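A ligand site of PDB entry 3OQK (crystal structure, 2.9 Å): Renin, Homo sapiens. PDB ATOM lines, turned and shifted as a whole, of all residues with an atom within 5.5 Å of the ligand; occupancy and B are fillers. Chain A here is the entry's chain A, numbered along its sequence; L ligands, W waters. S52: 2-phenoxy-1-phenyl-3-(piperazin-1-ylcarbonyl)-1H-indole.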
ATOM      1  N   THR A  18     -11.514  17.851 -20.813  1.00  0.00           N
ATOM      2  CA  THR A  18     -10.107  18.084 -20.498  1.00  0.00           C
ATOM      3  C   THR A  18      -9.168  16.998 -21.000  1.00  0.00           C
ATOM      4  O   THR A  18      -7.986  17.241 -21.169  1.00  0.00           O
ATOM      5  CB  THR A  18      -9.909  18.328 -19.001  1.00  0.00           C
ATOM      6  OG1 THR A  18     -10.383  17.197 -18.243  1.00  0.00           O
ATOM      7  CG2 THR A  18     -10.563  19.603 -18.535  1.00  0.00           C
ATOM      8  N   GLN A  19      -9.655  15.783 -21.160  1.00  0.00           N
ATOM      9  CA  GLN A  19      -8.813  14.678 -21.572  1.00  0.00           C
ATOM     10  C   GLN A  19      -9.488  13.950 -22.719  1.00  0.00           C
ATOM     11  O   GLN A  19     -10.627  13.514 -22.596  1.00  0.00           O
ATOM     12  CB  GLN A  19      -8.545  13.708 -20.412  1.00  0.00           C
ATOM     13  CG  GLN A  19      -7.922  14.378 -19.190  1.00  0.00           C
ATOM     14  CD  GLN A  19      -7.708  13.427 -18.072  1.00  0.00           C
ATOM     15  OE1 GLN A  19      -7.408  12.248 -18.283  1.00  0.00           O
ATOM     16  NE2 GLN A  19      -7.806  13.947 -16.840  1.00  0.00           N
ATOM     17  N   VAL A  36      -3.241   9.486 -24.871  1.00  0.00           N
ATOM     18  CA  VAL A  36      -3.454  10.818 -25.429  1.00  0.00           C
ATOM     19  C   VAL A  36      -2.557  10.876 -26.654  1.00  0.00           C
ATOM     20  O   VAL A  36      -1.402  10.400 -26.616  1.00  0.00           O
ATOM     21  CB  VAL A  36      -3.062  11.913 -24.421  1.00  0.00           C
ATOM     22  CG1 VAL A  36      -2.876  13.258 -25.093  1.00  0.00           C
ATOM     23  CG2 VAL A  36      -4.135  12.015 -23.353  1.00  0.00           C
ATOM     24  N   ASP A  38      -0.627  13.357 -28.734  1.00  0.00           N
ATOM     25  CA  ASP A  38      -0.063  14.648 -28.406  1.00  0.00           C
ATOM     26  C   ASP A  38       0.890  15.242 -29.451  1.00  0.00           C
ATOM     27  O   ASP A  38       2.009  14.764 -29.605  1.00  0.00           O
ATOM     28  CB  ASP A  38       0.640  14.518 -27.037  1.00  0.00           C
ATOM     29  CG  ASP A  38       1.357  15.752 -26.576  1.00  0.00           C
ATOM     30  OD1 ASP A  38       0.934  16.849 -26.945  1.00  0.00           O
ATOM     31  OD2 ASP A  38       2.330  15.618 -25.806  1.00  0.00           O
ATOM     32  N   GLY A  40       2.314  18.022 -29.198  1.00  0.00           N
ATOM     33  CA  GLY A  40       3.306  18.772 -28.456  1.00  0.00           C
ATOM     34  C   GLY A  40       4.542  17.984 -28.081  1.00  0.00           C
ATOM     35  O   GLY A  40       5.464  18.564 -27.512  1.00  0.00           O
ATOM     36  N   SER A  41       4.550  16.673 -28.345  1.00  0.00           N
ATOM     37  CA  SER A  41       5.676  15.800 -28.011  1.00  0.00           C
ATOM     38  C   SER A  41       5.811  14.714 -29.069  1.00  0.00           C
ATOM     39  O   SER A  41       4.949  14.558 -29.939  1.00  0.00           O
ATOM     40  CB  SER A  41       5.540  15.238 -26.593  1.00  0.00           C
ATOM     41  OG  SER A  41       4.472  14.314 -26.488  1.00  0.00           O
ATOM     42  N   TRP A  45       5.003   6.343 -24.889  1.00  0.00           N
ATOM     43  CA  TRP A  45       5.280   5.714 -23.611  1.00  0.00           C
ATOM     44  C   TRP A  45       3.998   5.204 -22.969  1.00  0.00           C
ATOM     45  O   TRP A  45       2.929   5.784 -23.142  1.00  0.00           O
ATOM     46  CB  TRP A  45       6.087   6.607 -22.636  1.00  0.00           C
ATOM     47  CG  TRP A  45       5.330   7.795 -22.098  1.00  0.00           C
ATOM     48  CD1 TRP A  45       5.386   9.071 -22.564  1.00  0.00           C
ATOM     49  CD2 TRP A  45       4.462   7.814 -20.947  1.00  0.00           C
ATOM     50  NE1 TRP A  45       4.587   9.890 -21.799  1.00  0.00           N
ATOM     51  CE2 TRP A  45       3.997   9.147 -20.800  1.00  0.00           C
ATOM     52  CE3 TRP A  45       3.985   6.839 -20.051  1.00  0.00           C
ATOM     53  CZ2 TRP A  45       3.116   9.524 -19.785  1.00  0.00           C
ATOM     54  CZ3 TRP A  45       3.122   7.226 -19.049  1.00  0.00           C
ATOM     55  CH2 TRP A  45       2.692   8.540 -18.925  1.00  0.00           C
ATOM     56  N   TYR A  83       7.771  16.896 -19.104  1.00  0.00           N
ATOM     57  CA  TYR A  83       6.647  17.642 -19.651  1.00  0.00           C
ATOM     58  C   TYR A  83       6.328  18.845 -18.815  1.00  0.00           C
ATOM     59  O   TYR A  83       6.844  18.964 -17.718  1.00  0.00           O
ATOM     60  CB  TYR A  83       5.398  16.745 -19.710  1.00  0.00           C
ATOM     61  CG  TYR A  83       5.560  15.536 -20.591  1.00  0.00           C
ATOM     62  CD1 TYR A  83       5.438  15.640 -21.982  1.00  0.00           C
ATOM     63  CD2 TYR A  83       5.798  14.285 -20.056  1.00  0.00           C
ATOM     64  CE1 TYR A  83       5.550  14.514 -22.801  1.00  0.00           C
ATOM     65  CE2 TYR A  83       5.914  13.152 -20.868  1.00  0.00           C
ATOM     66  CZ  TYR A  83       5.769  13.275 -22.245  1.00  0.00           C
ATOM     67  OH  TYR A  83       5.862  12.161 -23.043  1.00  0.00           O
ATOM     68  N   SER A  84       5.441  19.716 -19.316  1.00  0.00           N
ATOM     69  CA  SER A  84       5.013  20.921 -18.617  1.00  0.00           C
ATOM     70  C   SER A  84       4.350  20.625 -17.282  1.00  0.00           C
ATOM     71  O   SER A  84       4.493  21.393 -16.345  1.00  0.00           O
ATOM     72  CB  SER A  84       4.048  21.717 -19.491  1.00  0.00           C
ATOM     73  OG  SER A  84       4.789  22.241 -20.571  1.00  0.00           O
ATOM     74  N   THR A  85       3.624  19.506 -17.213  1.00  0.00           N
ATOM     75  CA  THR A  85       2.854  19.188 -16.023  1.00  0.00           C
ATOM     76  C   THR A  85       3.507  18.148 -15.109  1.00  0.00           C
ATOM     77  O   THR A  85       3.009  17.923 -13.995  1.00  0.00           O
ATOM     78  CB  THR A  85       1.439  18.792 -16.418  1.00  0.00           C
ATOM     79  OG1 THR A  85       1.520  17.666 -17.294  1.00  0.00           O
ATOM     80  CG2 THR A  85       0.688  19.904 -17.095  1.00  0.00           C
ATOM     81  N   GLY A  86       4.590  17.532 -15.554  1.00  0.00           N
ATOM     82  CA  GLY A  86       5.230  16.506 -14.768  1.00  0.00           C
ATOM     83  C   GLY A  86       6.297  15.783 -15.531  1.00  0.00           C
ATOM     84  O   GLY A  86       6.583  16.100 -16.685  1.00  0.00           O
ATOM     85  N   PRO A 118       1.088  14.678 -12.184  1.00  0.00           N
ATOM     86  CA  PRO A 118      -0.357  14.734 -12.512  1.00  0.00           C
ATOM     87  C   PRO A 118      -1.023  13.400 -12.829  1.00  0.00           C
ATOM     88  O   PRO A 118      -2.229  13.376 -13.087  1.00  0.00           O
ATOM     89  CB  PRO A 118      -0.350  15.575 -13.803  1.00  0.00           C
ATOM     90  CG  PRO A 118       0.931  15.157 -14.482  1.00  0.00           C
ATOM     91  CD  PRO A 118       1.920  14.748 -13.395  1.00  0.00           C
ATOM     92  N   PHE A 119      -0.261  12.304 -12.852  1.00  0.00           N
ATOM     93  CA  PHE A 119      -0.725  11.014 -13.377  1.00  0.00           C
ATOM     94  C   PHE A 119      -1.873  10.325 -12.680  1.00  0.00           C
ATOM     95  O   PHE A 119      -2.601   9.592 -13.333  1.00  0.00           O
ATOM     96  CB  PHE A 119       0.458  10.079 -13.782  1.00  0.00           C
ATOM     97  CG  PHE A 119       1.387  10.771 -14.779  1.00  0.00           C
ATOM     98  CD1 PHE A 119       0.992  10.985 -16.104  1.00  0.00           C
ATOM     99  CD2 PHE A 119       2.613  11.295 -14.358  1.00  0.00           C
ATOM    100  CE1 PHE A 119       1.822  11.681 -16.989  1.00  0.00           C
ATOM    101  CE2 PHE A 119       3.443  11.992 -15.257  1.00  0.00           C
ATOM    102  CZ  PHE A 119       3.041  12.176 -16.563  1.00  0.00           C
ATOM    103  N   LEU A 121      -4.403  11.939 -11.872  1.00  0.00           N
ATOM    104  CA  LEU A 121      -5.529  12.708 -12.410  1.00  0.00           C
ATOM    105  C   LEU A 121      -5.814  12.331 -13.859  1.00  0.00           C
ATOM    106  O   LEU A 121      -6.768  12.843 -14.466  1.00  0.00           O
ATOM    107  CB  LEU A 121      -5.266  14.221 -12.293  1.00  0.00           C
ATOM    108  CG  LEU A 121      -4.908  14.757 -10.906  1.00  0.00           C
ATOM    109  CD1 LEU A 121      -4.111  16.054 -10.971  1.00  0.00           C
ATOM    110  CD2 LEU A 121      -6.056  14.674  -9.934  1.00  0.00           C
ATOM    111  N   ALA A 122      -4.967  11.473 -14.420  1.00  0.00           N
ATOM    112  CA  ALA A 122      -5.076  11.046 -15.812  1.00  0.00           C
ATOM    113  C   ALA A 122      -5.985   9.842 -15.956  1.00  0.00           C
ATOM    114  O   ALA A 122      -5.763   8.813 -15.316  1.00  0.00           O
ATOM    115  CB  ALA A 122      -3.678  10.739 -16.385  1.00  0.00           C
ATOM    116  N   PHE A 124      -6.142   8.485 -18.874  1.00  0.00           N
ATOM    117  CA  PHE A 124      -5.351   7.736 -19.834  1.00  0.00           C
ATOM    118  C   PHE A 124      -4.147   7.102 -19.145  1.00  0.00           C
ATOM    119  O   PHE A 124      -3.737   7.553 -18.073  1.00  0.00           O
ATOM    120  CB  PHE A 124      -4.889   8.674 -20.965  1.00  0.00           C
ATOM    121  CG  PHE A 124      -4.132   9.898 -20.504  1.00  0.00           C
ATOM    122  CD1 PHE A 124      -4.827  11.074 -20.156  1.00  0.00           C
ATOM    123  CD2 PHE A 124      -2.738   9.890 -20.415  1.00  0.00           C
ATOM    124  CE1 PHE A 124      -4.130  12.225 -19.750  1.00  0.00           C
ATOM    125  CE2 PHE A 124      -2.038  11.035 -19.987  1.00  0.00           C
ATOM    126  CZ  PHE A 124      -2.743  12.189 -19.670  1.00  0.00           C
ATOM    127  N   VAL A 127       1.018   8.100 -23.490  1.00  0.00           N
ATOM    128  CA  VAL A 127       1.038   9.138 -24.494  1.00  0.00           C
ATOM    129  C   VAL A 127       1.577   8.596 -25.792  1.00  0.00           C
ATOM    130  O   VAL A 127       2.552   7.832 -25.794  1.00  0.00           O
ATOM    131  CB  VAL A 127       1.887  10.381 -24.017  1.00  0.00           C
ATOM    132  CG1 VAL A 127       1.895  11.503 -25.051  1.00  0.00           C
ATOM    133  CG2 VAL A 127       1.368  10.924 -22.668  1.00  0.00           C
ATOM    134  N   ASP A 226      -1.252  22.206 -29.882  1.00  0.00           N
ATOM    135  CA  ASP A 226      -0.995  21.133 -28.947  1.00  0.00           C
ATOM    136  C   ASP A 226      -2.198  20.321 -28.534  1.00  0.00           C
ATOM    137  O   ASP A 226      -2.924  20.694 -27.616  1.00  0.00           O
ATOM    138  CB  ASP A 226      -0.327  21.764 -27.713  1.00  0.00           C
ATOM    139  CG  ASP A 226       0.347  20.810 -26.816  1.00  0.00           C
ATOM    140  OD1 ASP A 226       0.270  19.589 -27.083  1.00  0.00           O
ATOM    141  OD2 ASP A 226       0.979  21.262 -25.854  1.00  0.00           O
ATOM    142  N   GLY A 228      -2.342  17.611 -26.924  1.00  0.00           N
ATOM    143  CA  GLY A 228      -2.132  17.015 -25.609  1.00  0.00           C
ATOM    144  C   GLY A 228      -2.364  17.959 -24.461  1.00  0.00           C
ATOM    145  O   GLY A 228      -2.303  17.538 -23.302  1.00  0.00           O
ATOM    146  N   ALA A 229      -2.631  19.222 -24.748  1.00  0.00           N
ATOM    147  CA  ALA A 229      -2.880  20.228 -23.725  1.00  0.00           C
ATOM    148  C   ALA A 229      -4.397  20.415 -23.578  1.00  0.00           C
ATOM    149  O   ALA A 229      -5.094  20.506 -24.588  1.00  0.00           O
ATOM    150  CB  ALA A 229      -2.215  21.539 -24.110  1.00  0.00           C
ATOM    151  N   SER A 230      -4.913  20.476 -22.342  1.00  0.00           N
ATOM    152  CA  SER A 230      -6.351  20.639 -22.125  1.00  0.00           C
ATOM    153  C   SER A 230      -6.839  22.030 -22.443  1.00  0.00           C
ATOM    154  O   SER A 230      -7.983  22.174 -22.896  1.00  0.00           O
ATOM    155  CB  SER A 230      -6.735  20.350 -20.673  1.00  0.00           C
ATOM    156  OG  SER A 230      -6.346  19.045 -20.281  1.00  0.00           O
ATOM    157  N   TYR A 231      -5.998  23.046 -22.241  1.00  0.00           N
ATOM    158  CA  TYR A 231      -6.393  24.442 -22.394  1.00  0.00           C
ATOM    159  C   TYR A 231      -5.610  25.231 -23.416  1.00  0.00           C
ATOM    160  O   TYR A 231      -4.669  24.740 -24.054  1.00  0.00           O
ATOM    161  CB  TYR A 231      -6.263  25.116 -21.009  1.00  0.00           C
ATOM    162  CG  TYR A 231      -6.846  24.289 -19.873  1.00  0.00           C
ATOM    163  CD1 TYR A 231      -6.027  23.763 -18.886  1.00  0.00           C
ATOM    164  CD2 TYR A 231      -8.207  23.967 -19.838  1.00  0.00           C
ATOM    165  CE1 TYR A 231      -6.556  22.971 -17.861  1.00  0.00           C
ATOM    166  CE2 TYR A 231      -8.743  23.188 -18.812  1.00  0.00           C
ATOM    167  CZ  TYR A 231      -7.914  22.684 -17.824  1.00  0.00           C
ATOM    168  OH  TYR A 231      -8.458  21.902 -16.841  1.00  0.00           O
ATOM    169  N   HIS A 301      -5.057  29.088 -19.183  1.00  0.00           N
ATOM    170  CA  HIS A 301      -4.192  29.175 -18.012  1.00  0.00           C
ATOM    171  C   HIS A 301      -2.756  29.570 -18.354  1.00  0.00           C
ATOM    172  O   HIS A 301      -2.401  29.667 -19.534  1.00  0.00           O
ATOM    173  CB  HIS A 301      -4.291  27.902 -17.136  1.00  0.00           C
ATOM    174  CG  HIS A 301      -3.687  26.662 -17.722  1.00  0.00           C
ATOM    175  ND1 HIS A 301      -3.529  25.533 -16.955  1.00  0.00           N
ATOM    176  CD2 HIS A 301      -3.214  26.414 -18.969  1.00  0.00           C
ATOM    177  CE1 HIS A 301      -2.977  24.624 -17.756  1.00  0.00           C
ATOM    178  NE2 HIS A 301      -2.755  25.120 -18.972  1.00  0.00           N
ATOM    179  N   MET A 303       1.141  28.832 -18.620  1.00  0.00           N
ATOM    180  CA  MET A 303       2.092  27.735 -18.754  1.00  0.00           C
ATOM    181  C   MET A 303       3.343  28.260 -19.409  1.00  0.00           C
ATOM    182  O   MET A 303       3.314  28.667 -20.570  1.00  0.00           O
ATOM    183  CB  MET A 303       1.523  26.527 -19.517  1.00  0.00           C
ATOM    184  CG  MET A 303       2.261  25.246 -19.218  1.00  0.00           C
ATOM    185  SD  MET A 303       1.409  24.329 -17.871  1.00  0.00           S
ATOM    186  CE  MET A 303       0.312  23.413 -18.765  1.00  0.00           C
HETATM  187  C1  S52 L   1      -4.400  14.967 -16.639  1.00  0.00           C
HETATM  188  O1  S52 L   1      -0.264  15.888 -19.401  1.00  0.00           O
HETATM  189  C2  S52 L   1      -5.031  15.826 -17.562  1.00  0.00           C
HETATM  190  C3  S52 L   1      -4.243  16.633 -18.392  1.00  0.00           C
HETATM  191  C4  S52 L   1      -2.811  16.640 -18.337  1.00  0.00           C
HETATM  192  C5  S52 L   1      -2.248  15.773 -17.358  1.00  0.00           C
HETATM  193  C6  S52 L   1      -3.005  14.935 -16.544  1.00  0.00           C
HETATM  194  N12 S52 L   1      -1.999  17.457 -19.067  1.00  0.00           N
HETATM  195  C13 S52 L   1      -2.216  18.784 -19.243  1.00  0.00           C
HETATM  196  C14 S52 L   1      -1.057  19.290 -19.914  1.00  0.00           C
HETATM  197  C15 S52 L   1      -0.186  18.214 -20.077  1.00  0.00           C
HETATM  198  C16 S52 L   1      -0.776  17.139 -19.472  1.00  0.00           C
HETATM  199  C17 S52 L   1      -3.299  19.636 -18.983  1.00  0.00           C
HETATM  200  C18 S52 L   1      -3.204  20.980 -19.373  1.00  0.00           C
HETATM  201  C19 S52 L   1      -2.065  21.458 -20.033  1.00  0.00           C
HETATM  202  C20 S52 L   1      -0.977  20.617 -20.299  1.00  0.00           C
HETATM  203  C26 S52 L   1       0.402  15.325 -20.458  1.00  0.00           C
HETATM  204  C29 S52 L   1       1.671  14.774 -20.210  1.00  0.00           C
HETATM  205  C30 S52 L   1       2.361  14.194 -21.296  1.00  0.00           C
HETATM  206  C31 S52 L   1       1.809  14.194 -22.585  1.00  0.00           C
HETATM  207  C32 S52 L   1       0.553  14.759 -22.797  1.00  0.00           C
HETATM  208  C33 S52 L   1      -0.157  15.337 -21.732  1.00  0.00           C
HETATM  209  C39 S52 L   1       1.218  18.300 -20.627  1.00  0.00           C
HETATM  210  N40 S52 L   1       1.579  18.753 -21.851  1.00  0.00           N
HETATM  211  O41 S52 L   1       2.090  17.894 -19.803  1.00  0.00           O
HETATM  212  C42 S52 L   1       0.668  19.245 -22.883  1.00  0.00           C
HETATM  213  C43 S52 L   1       0.852  18.392 -24.140  1.00  0.00           C
HETATM  214  N44 S52 L   1       2.232  18.094 -24.429  1.00  0.00           N
HETATM  215  C45 S52 L   1       3.123  17.734 -23.332  1.00  0.00           C
HETATM  216  C46 S52 L   1       2.998  18.757 -22.207  1.00  0.00           C
HETATM  217  O   HOH W   1       6.092  19.676 -22.256  1.00  0.00           O
HETATM  218  O   HOH W   2      -3.128  24.152 -21.716  1.00  0.00           O
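Water W2 lies within hydrogen-bond range of the backbone carbonyl oxygen of Tyr 231 and a ring nitrogen (NE2) of His 301.
O41 of the ligand is in hydrogen-bond range of N of Thr 85 (3.4 Å). OG1 of Thr 85 sits at hydrogen-bond distance from O41 of the ligand (2.6 Å). The side-chain carboxylate (OD2) of Asp 38 lies within salt-bridge range of a nitrogen (N44) of the ligand (2.8 Å). The side-chain carboxylate (OD1) of Asp 226 lies within salt-bridge range of a nitrogen (N44) of the ligand (3.6 Å).
Merely in contact with the ligand: Gln 19 (3.4 Å), Tyr 83 (3.4 Å), Ser 84 (3.8 Å), Pro 118 (3.9 Å), Leu 121 (3.9 Å), Val 127 (3.3 Å), Gly 228 (3.3 Å), Ala 229 (3.6 Å), Ser 230 (3.4 Å), Tyr 231 (3.99 Å), His 301 (3.9 Å) and Met 303 (3.3 Å). Hydrophobic or aromatic side chains within 4 Å of the ligand: Tyr 83, Pro 118, Val 127, Ala 229, Tyr 231, His 301 and Met 303. 15 residues have an atom within 4 Å of the ligand: Gln 19, Asp 38, Tyr 83, Ser 84, Thr 85, Pro 118, Leu 121, Val 127, Asp 226, Gly 228, Ala 229, Ser 230, Tyr 231, His 301 and Met 303. The nearest printed residue that does not touch the ligand is Ala 122 (4.1 Å).
N of Gly 228 sits close to OD1 of Asp 38. The side-chain carboxylate (OD1) of Asp 38 sits at hydrogen-bond distance from the backbone NH (N) of Gly 40. The side-chain hydroxyl (OG) of Ser 41 lies within hydrogen-bond range of the side-chain carboxylate (OD2) of Asp 38 (2.6 Å). OD1 of Asp 226 lies close to N of Gly 228 (3.3 Å). OD1 of Asp 226 is in hydrogen-bond range of N of Gly 40 (3.3 Å). The side-chain hydroxyl of Ser 230 lies within hydrogen-bond range of the backbone carbonyl oxygen of Thr 18 (2.6 Å). OH of Tyr 83 lies within hydrogen-bond range of NE1 of Trp 45 (2.9 Å). The backbone carbonyl oxygen of Leu 121 lies within hydrogen-bond range of the side-chain amide nitrogen of Gln 19, at 2.8 Å.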
